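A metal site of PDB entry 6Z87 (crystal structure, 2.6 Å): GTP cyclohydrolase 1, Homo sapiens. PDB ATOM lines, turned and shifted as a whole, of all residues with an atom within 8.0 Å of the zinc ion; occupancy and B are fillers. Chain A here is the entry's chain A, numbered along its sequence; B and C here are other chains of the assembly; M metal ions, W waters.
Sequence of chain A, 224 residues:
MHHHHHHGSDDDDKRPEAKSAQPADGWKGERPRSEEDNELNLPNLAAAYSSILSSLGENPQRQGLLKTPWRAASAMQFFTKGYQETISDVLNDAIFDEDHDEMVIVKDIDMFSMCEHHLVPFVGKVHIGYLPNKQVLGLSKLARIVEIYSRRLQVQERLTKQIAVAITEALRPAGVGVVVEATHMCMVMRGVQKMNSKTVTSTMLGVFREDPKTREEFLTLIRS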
ATOM      1  N   MET A 114       8.744  -8.744 -35.305  1.00  0.00           N
ATOM      2  CA  MET A 114       9.002  -9.109 -33.922  1.00  0.00           C
ATOM      3  C   MET A 114       7.816  -8.782 -33.058  1.00  0.00           C
ATOM      4  O   MET A 114       7.337  -7.660 -33.075  1.00  0.00           O
ATOM      5  CB  MET A 114      10.217  -8.349 -33.397  1.00  0.00           C
ATOM      6  CG  MET A 114      11.521  -8.912 -33.868  1.00  0.00           C
ATOM      7  SD  MET A 114      11.921 -10.456 -32.999  1.00  0.00           S
ATOM      8  CE  MET A 114      11.877  -9.867 -31.401  1.00  0.00           C
ATOM      9  N   CYS A 115       7.338  -9.744 -32.279  1.00  0.00           N
ATOM     10  CA  CYS A 115       6.241  -9.570 -31.338  1.00  0.00           C
ATOM     11  C   CYS A 115       6.683  -8.542 -30.281  1.00  0.00           C
ATOM     12  O   CYS A 115       7.782  -8.679 -29.741  1.00  0.00           O
ATOM     13  CB  CYS A 115       5.926 -10.917 -30.692  1.00  0.00           C
ATOM     14  SG  CYS A 115       4.725 -10.833 -29.340  1.00  0.00           S
ATOM     15  N   GLU A 116       5.875  -7.500 -30.039  1.00  0.00           N
ATOM     16  CA  GLU A 116       6.258  -6.511 -29.025  1.00  0.00           C
ATOM     17  C   GLU A 116       5.952  -6.973 -27.616  1.00  0.00           C
ATOM     18  O   GLU A 116       6.481  -6.371 -26.676  1.00  0.00           O
ATOM     19  CB  GLU A 116       5.636  -5.145 -29.292  1.00  0.00           C
ATOM     20  CG  GLU A 116       4.141  -5.105 -28.999  1.00  0.00           C
ATOM     21  CD  GLU A 116       3.470  -3.804 -29.356  1.00  0.00           C
ATOM     22  OE1 GLU A 116       4.070  -3.004 -30.109  1.00  0.00           O
ATOM     23  OE2 GLU A 116       2.336  -3.581 -28.865  1.00  0.00           O
ATOM     24  N   HIS A 117       5.090  -7.993 -27.433  1.00  0.00           N
ATOM     25  CA  HIS A 117       4.773  -8.461 -26.094  1.00  0.00           C
ATOM     26  C   HIS A 117       5.824  -9.409 -25.533  1.00  0.00           C
ATOM     27  O   HIS A 117       6.133  -9.324 -24.339  1.00  0.00           O
ATOM     28  CB  HIS A 117       3.408  -9.137 -26.044  1.00  0.00           C
ATOM     29  CG  HIS A 117       2.308  -8.245 -26.509  1.00  0.00           C
ATOM     30  ND1 HIS A 117       1.323  -8.706 -27.339  1.00  0.00           N
ATOM     31  CD2 HIS A 117       2.095  -6.942 -26.249  1.00  0.00           C
ATOM     32  CE1 HIS A 117       0.520  -7.679 -27.550  1.00  0.00           C
ATOM     33  NE2 HIS A 117       0.951  -6.581 -26.921  1.00  0.00           N
ATOM     34  N   HIS A 118       6.362 -10.300 -26.371  1.00  0.00           N
ATOM     35  CA  HIS A 118       7.307 -11.295 -25.897  1.00  0.00           C
ATOM     36  C   HIS A 118       8.682 -11.235 -26.530  1.00  0.00           C
ATOM     37  O   HIS A 118       9.551 -12.020 -26.146  1.00  0.00           O
ATOM     38  CB  HIS A 118       6.748 -12.712 -26.114  1.00  0.00           C
ATOM     39  CG  HIS A 118       5.396 -12.928 -25.503  1.00  0.00           C
ATOM     40  ND1 HIS A 118       4.240 -12.755 -26.243  1.00  0.00           N
ATOM     41  CD2 HIS A 118       5.064 -13.281 -24.234  1.00  0.00           C
ATOM     42  CE1 HIS A 118       3.233 -13.006 -25.407  1.00  0.00           C
ATOM     43  NE2 HIS A 118       3.682 -13.328 -24.187  1.00  0.00           N
ATOM     44  N   LEU A 119       8.888 -10.356 -27.515  1.00  0.00           N
ATOM     45  CA  LEU A 119      10.164 -10.243 -28.235  1.00  0.00           C
ATOM     46  C   LEU A 119      10.538 -11.538 -28.945  1.00  0.00           C
ATOM     47  O   LEU A 119      11.709 -11.929 -28.958  1.00  0.00           O
ATOM     48  CB  LEU A 119      11.319  -9.707 -27.381  1.00  0.00           C
ATOM     49  CG  LEU A 119      11.060  -8.385 -26.676  1.00  0.00           C
ATOM     50  CD1 LEU A 119      12.247  -8.006 -25.838  1.00  0.00           C
ATOM     51  CD2 LEU A 119      10.724  -7.275 -27.661  1.00  0.00           C
ATOM     52  N   VAL A 120       9.522 -12.193 -29.527  1.00  0.00           N
ATOM     53  CA  VAL A 120       9.658 -13.436 -30.290  1.00  0.00           C
ATOM     54  C   VAL A 120       9.160 -13.130 -31.710  1.00  0.00           C
ATOM     55  O   VAL A 120       8.130 -12.488 -31.869  1.00  0.00           O
ATOM     56  CB  VAL A 120       8.818 -14.563 -29.634  1.00  0.00           C
ATOM     57  CG1 VAL A 120       9.023 -15.879 -30.342  1.00  0.00           C
ATOM     58  CG2 VAL A 120       9.157 -14.726 -28.165  1.00  0.00           C
ATOM     59  N   PRO A 121       9.857 -13.614 -32.758  1.00  0.00           N
ATOM     60  CA  PRO A 121       9.392 -13.337 -34.136  1.00  0.00           C
ATOM     61  C   PRO A 121       7.981 -13.806 -34.496  1.00  0.00           C
ATOM     62  O   PRO A 121       7.389 -14.643 -33.812  1.00  0.00           O
ATOM     63  CB  PRO A 121      10.432 -14.083 -35.005  1.00  0.00           C
ATOM     64  CG  PRO A 121      11.637 -14.192 -34.174  1.00  0.00           C
ATOM     65  CD  PRO A 121      11.102 -14.397 -32.766  1.00  0.00           C
ATOM     66  N   PHE A 122       7.423 -13.224 -35.551  1.00  0.00           N
ATOM     67  CA  PHE A 122       6.177 -13.636 -36.177  1.00  0.00           C
ATOM     68  C   PHE A 122       6.375 -13.372 -37.664  1.00  0.00           C
ATOM     69  O   PHE A 122       6.752 -12.269 -38.055  1.00  0.00           O
ATOM     70  CB  PHE A 122       4.896 -13.049 -35.543  1.00  0.00           C
ATOM     71  CG  PHE A 122       4.587 -11.589 -35.731  1.00  0.00           C
ATOM     72  CD1 PHE A 122       3.823 -11.159 -36.815  1.00  0.00           C
ATOM     73  CD2 PHE A 122       4.973 -10.648 -34.798  1.00  0.00           C
ATOM     74  CE1 PHE A 122       3.528  -9.809 -36.980  1.00  0.00           C
ATOM     75  CE2 PHE A 122       4.683  -9.299 -34.972  1.00  0.00           C
ATOM     76  CZ  PHE A 122       3.947  -8.902 -36.049  1.00  0.00           C
ATOM     77  N   GLN A 154       6.269  -5.034 -32.949  1.00  0.00           N
ATOM     78  CA  GLN A 154       4.926  -4.868 -33.463  1.00  0.00           C
ATOM     79  C   GLN A 154       3.817  -5.739 -32.862  1.00  0.00           C
ATOM     80  O   GLN A 154       4.057  -6.679 -32.093  1.00  0.00           O
ATOM     81  CB  GLN A 154       4.983  -5.189 -34.984  1.00  0.00           C
ATOM     82  CG  GLN A 154       5.475  -4.044 -35.840  1.00  0.00           C
ATOM     83  CD  GLN A 154       4.429  -2.980 -36.049  1.00  0.00           C
ATOM     84  OE1 GLN A 154       3.365  -2.954 -35.428  1.00  0.00           O
ATOM     85  NE2 GLN A 154       4.724  -2.071 -36.940  1.00  0.00           N
ATOM     86  N   VAL A 155       2.581  -5.391 -33.252  1.00  0.00           N
ATOM     87  CA  VAL A 155       1.360  -6.160 -33.076  1.00  0.00           C
ATOM     88  C   VAL A 155       0.841  -6.246 -34.502  1.00  0.00           C
ATOM     89  O   VAL A 155       0.813  -5.233 -35.216  1.00  0.00           O
ATOM     90  CB  VAL A 155       0.319  -5.604 -32.089  1.00  0.00           C
ATOM     91  CG1 VAL A 155       0.673  -5.956 -30.675  1.00  0.00           C
ATOM     92  CG2 VAL A 155       0.106  -4.131 -32.245  1.00  0.00           C
ATOM     93  N   HIS A 184       2.796 -16.811 -35.417  1.00  0.00           N
ATOM     94  CA  HIS A 184       3.414 -16.205 -34.246  1.00  0.00           C
ATOM     95  C   HIS A 184       4.209 -17.247 -33.490  1.00  0.00           C
ATOM     96  O   HIS A 184       3.634 -18.196 -32.993  1.00  0.00           O
ATOM     97  CB  HIS A 184       2.335 -15.564 -33.357  1.00  0.00           C
ATOM     98  CG  HIS A 184       1.725 -14.335 -33.965  1.00  0.00           C
ATOM     99  ND1 HIS A 184       1.764 -13.122 -33.316  1.00  0.00           N
ATOM    100  CD2 HIS A 184       1.128 -14.169 -35.176  1.00  0.00           C
ATOM    101  CE1 HIS A 184       1.196 -12.254 -34.150  1.00  0.00           C
ATOM    102  NE2 HIS A 184       0.797 -12.838 -35.266  1.00  0.00           N
ATOM    103  N   MET A 185       5.538 -17.081 -33.413  1.00  0.00           N
ATOM    104  CA  MET A 185       6.395 -18.046 -32.728  1.00  0.00           C
ATOM    105  C   MET A 185       6.137 -18.080 -31.226  1.00  0.00           C
ATOM    106  O   MET A 185       6.354 -19.123 -30.609  1.00  0.00           O
ATOM    107  CB  MET A 185       7.884 -17.810 -32.998  1.00  0.00           C
ATOM    108  CG  MET A 185       8.210 -17.657 -34.442  1.00  0.00           C
ATOM    109  SD  MET A 185       8.450 -19.209 -35.254  1.00  0.00           S
ATOM    110  CE  MET A 185       7.372 -18.980 -36.657  1.00  0.00           C
ATOM    111  N   CYS A 186       5.663 -16.978 -30.634  1.00  0.00           N
ATOM    112  CA  CYS A 186       5.395 -16.936 -29.194  1.00  0.00           C
ATOM    113  C   CYS A 186       4.294 -17.913 -28.739  1.00  0.00           C
ATOM    114  O   CYS A 186       4.169 -18.174 -27.542  1.00  0.00           O
ATOM    115  CB  CYS A 186       5.126 -15.514 -28.710  1.00  0.00           C
ATOM    116  SG  CYS A 186       4.134 -14.499 -29.846  1.00  0.00           S
ATOM    117  N   MET A 187       3.546 -18.502 -29.684  1.00  0.00           N
ATOM    118  CA  MET A 187       2.546 -19.492 -29.348  1.00  0.00           C
ATOM    119  C   MET A 187       2.802 -20.838 -30.095  1.00  0.00           C
ATOM    120  O   MET A 187       2.334 -21.872 -29.623  1.00  0.00           O
ATOM    121  CB  MET A 187       1.115 -18.941 -29.538  1.00  0.00           C
ATOM    122  CG  MET A 187       0.707 -18.788 -30.981  1.00  0.00           C
ATOM    123  SD  MET A 187      -1.064 -18.529 -31.332  1.00  0.00           S
ATOM    124  CE  MET A 187      -1.859 -19.259 -29.889  1.00  0.00           C
ATOM    125  N   ARG A 190       5.043 -22.689 -27.964  1.00  0.00           N
ATOM    126  CA  ARG A 190       4.278 -23.190 -26.832  1.00  0.00           C
ATOM    127  C   ARG A 190       3.332 -24.386 -27.187  1.00  0.00           C
ATOM    128  O   ARG A 190       2.559 -24.843 -26.333  1.00  0.00           O
ATOM    129  CB  ARG A 190       3.520 -22.028 -26.149  1.00  0.00           C
ATOM    130  CG  ARG A 190       4.200 -21.570 -24.871  1.00  0.00           C
ATOM    131  CD  ARG A 190       3.725 -20.218 -24.407  1.00  0.00           C
ATOM    132  NE  ARG A 190       4.561 -19.112 -24.872  1.00  0.00           N
ATOM    133  CZ  ARG A 190       5.326 -18.350 -24.101  1.00  0.00           C
ATOM    134  NH1 ARG A 190       5.370 -18.557 -22.788  1.00  0.00           N
ATOM    135  NH2 ARG A 190       6.039 -17.368 -24.628  1.00  0.00           N
ATOM    136  N   LEU B 139      -3.409 -13.441 -28.287  1.00  0.00           N
ATOM    137  CA  LEU B 139      -3.455 -14.702 -29.022  1.00  0.00           C
ATOM    138  C   LEU B 139      -3.368 -15.901 -28.084  1.00  0.00           C
ATOM    139  O   LEU B 139      -4.068 -16.886 -28.277  1.00  0.00           O
ATOM    140  CB  LEU B 139      -2.306 -14.766 -30.032  1.00  0.00           C
ATOM    141  CG  LEU B 139      -2.583 -14.325 -31.480  1.00  0.00           C
ATOM    142  CD1 LEU B 139      -3.338 -12.998 -31.568  1.00  0.00           C
ATOM    143  CD2 LEU B 139      -1.292 -14.199 -32.251  1.00  0.00           C
ATOM    144  N   SER B 140      -2.523 -15.799 -27.054  1.00  0.00           N
ATOM    145  CA  SER B 140      -2.364 -16.881 -26.067  1.00  0.00           C
ATOM    146  C   SER B 140      -3.648 -17.076 -25.271  1.00  0.00           C
ATOM    147  O   SER B 140      -4.003 -18.208 -24.954  1.00  0.00           O
ATOM    148  CB  SER B 140      -1.198 -16.580 -25.127  1.00  0.00           C
ATOM    149  OG  SER B 140      -0.028 -16.244 -25.853  1.00  0.00           O
ATOM    150  N   ARG C  71       7.173 -10.384 -19.659  1.00  0.00           N
ATOM    151  CA  ARG C  71       6.666 -11.355 -20.622  1.00  0.00           C
ATOM    152  C   ARG C  71       7.798 -12.010 -21.394  1.00  0.00           C
ATOM    153  O   ARG C  71       7.762 -13.211 -21.609  1.00  0.00           O
ATOM    154  CB  ARG C  71       5.695 -10.689 -21.593  1.00  0.00           C
ATOM    155  CG  ARG C  71       4.337 -10.432 -21.001  1.00  0.00           C
ATOM    156  CD  ARG C  71       3.380 -10.075 -22.109  1.00  0.00           C
ATOM    157  NE  ARG C  71       3.679  -8.769 -22.680  1.00  0.00           N
ATOM    158  CZ  ARG C  71       2.820  -7.746 -22.682  1.00  0.00           C
ATOM    159  NH1 ARG C  71       1.599  -7.896 -22.175  1.00  0.00           N
ATOM    160  NH2 ARG C  71       3.171  -6.572 -23.196  1.00  0.00           N
ATOM    161  N   ALA C  75       9.027 -15.898 -21.230  1.00  0.00           N
ATOM    162  CA  ALA C  75       9.081 -16.645 -22.475  1.00  0.00           C
ATOM    163  C   ALA C  75      10.459 -17.273 -22.600  1.00  0.00           C
ATOM    164  O   ALA C  75      10.537 -18.450 -22.865  1.00  0.00           O
ATOM    165  CB  ALA C  75       8.806 -15.733 -23.659  1.00  0.00           C
HETATM  166 ZN    ZN M   1       3.894 -12.688 -28.380  1.00  0.00          ZN
HETATM  167  O   HOH W   1       1.275 -11.684 -29.277  1.00  0.00           O
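The guanidinium group of Arg 190 sits at hydrogen-bond distance from the backbone carbonyl oxygen of Cys 186, 2.9 Å away.
The backbone NH of Cys 115 is in hydrogen-bond range of the backbone carbonyl oxygen of Val 120 (2.9 Å).
SG of Cys 115 lies close to N of His 117, at 3.4 Å.
Along chain A the residues within 4 Å of the zinc ion span positions 115 to 186.
The nearest printed residue that does not touch the zinc ion is His 117 (4.3 Å).
The zinc ion is bound by a ring nitrogen (ND1) of His 118 (2.2 Å), the side-chain sulfur (SG) of Cys 115 (2.2 Å) and the side-chain sulfur (SG) of Cys 186 (2.3 Å).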
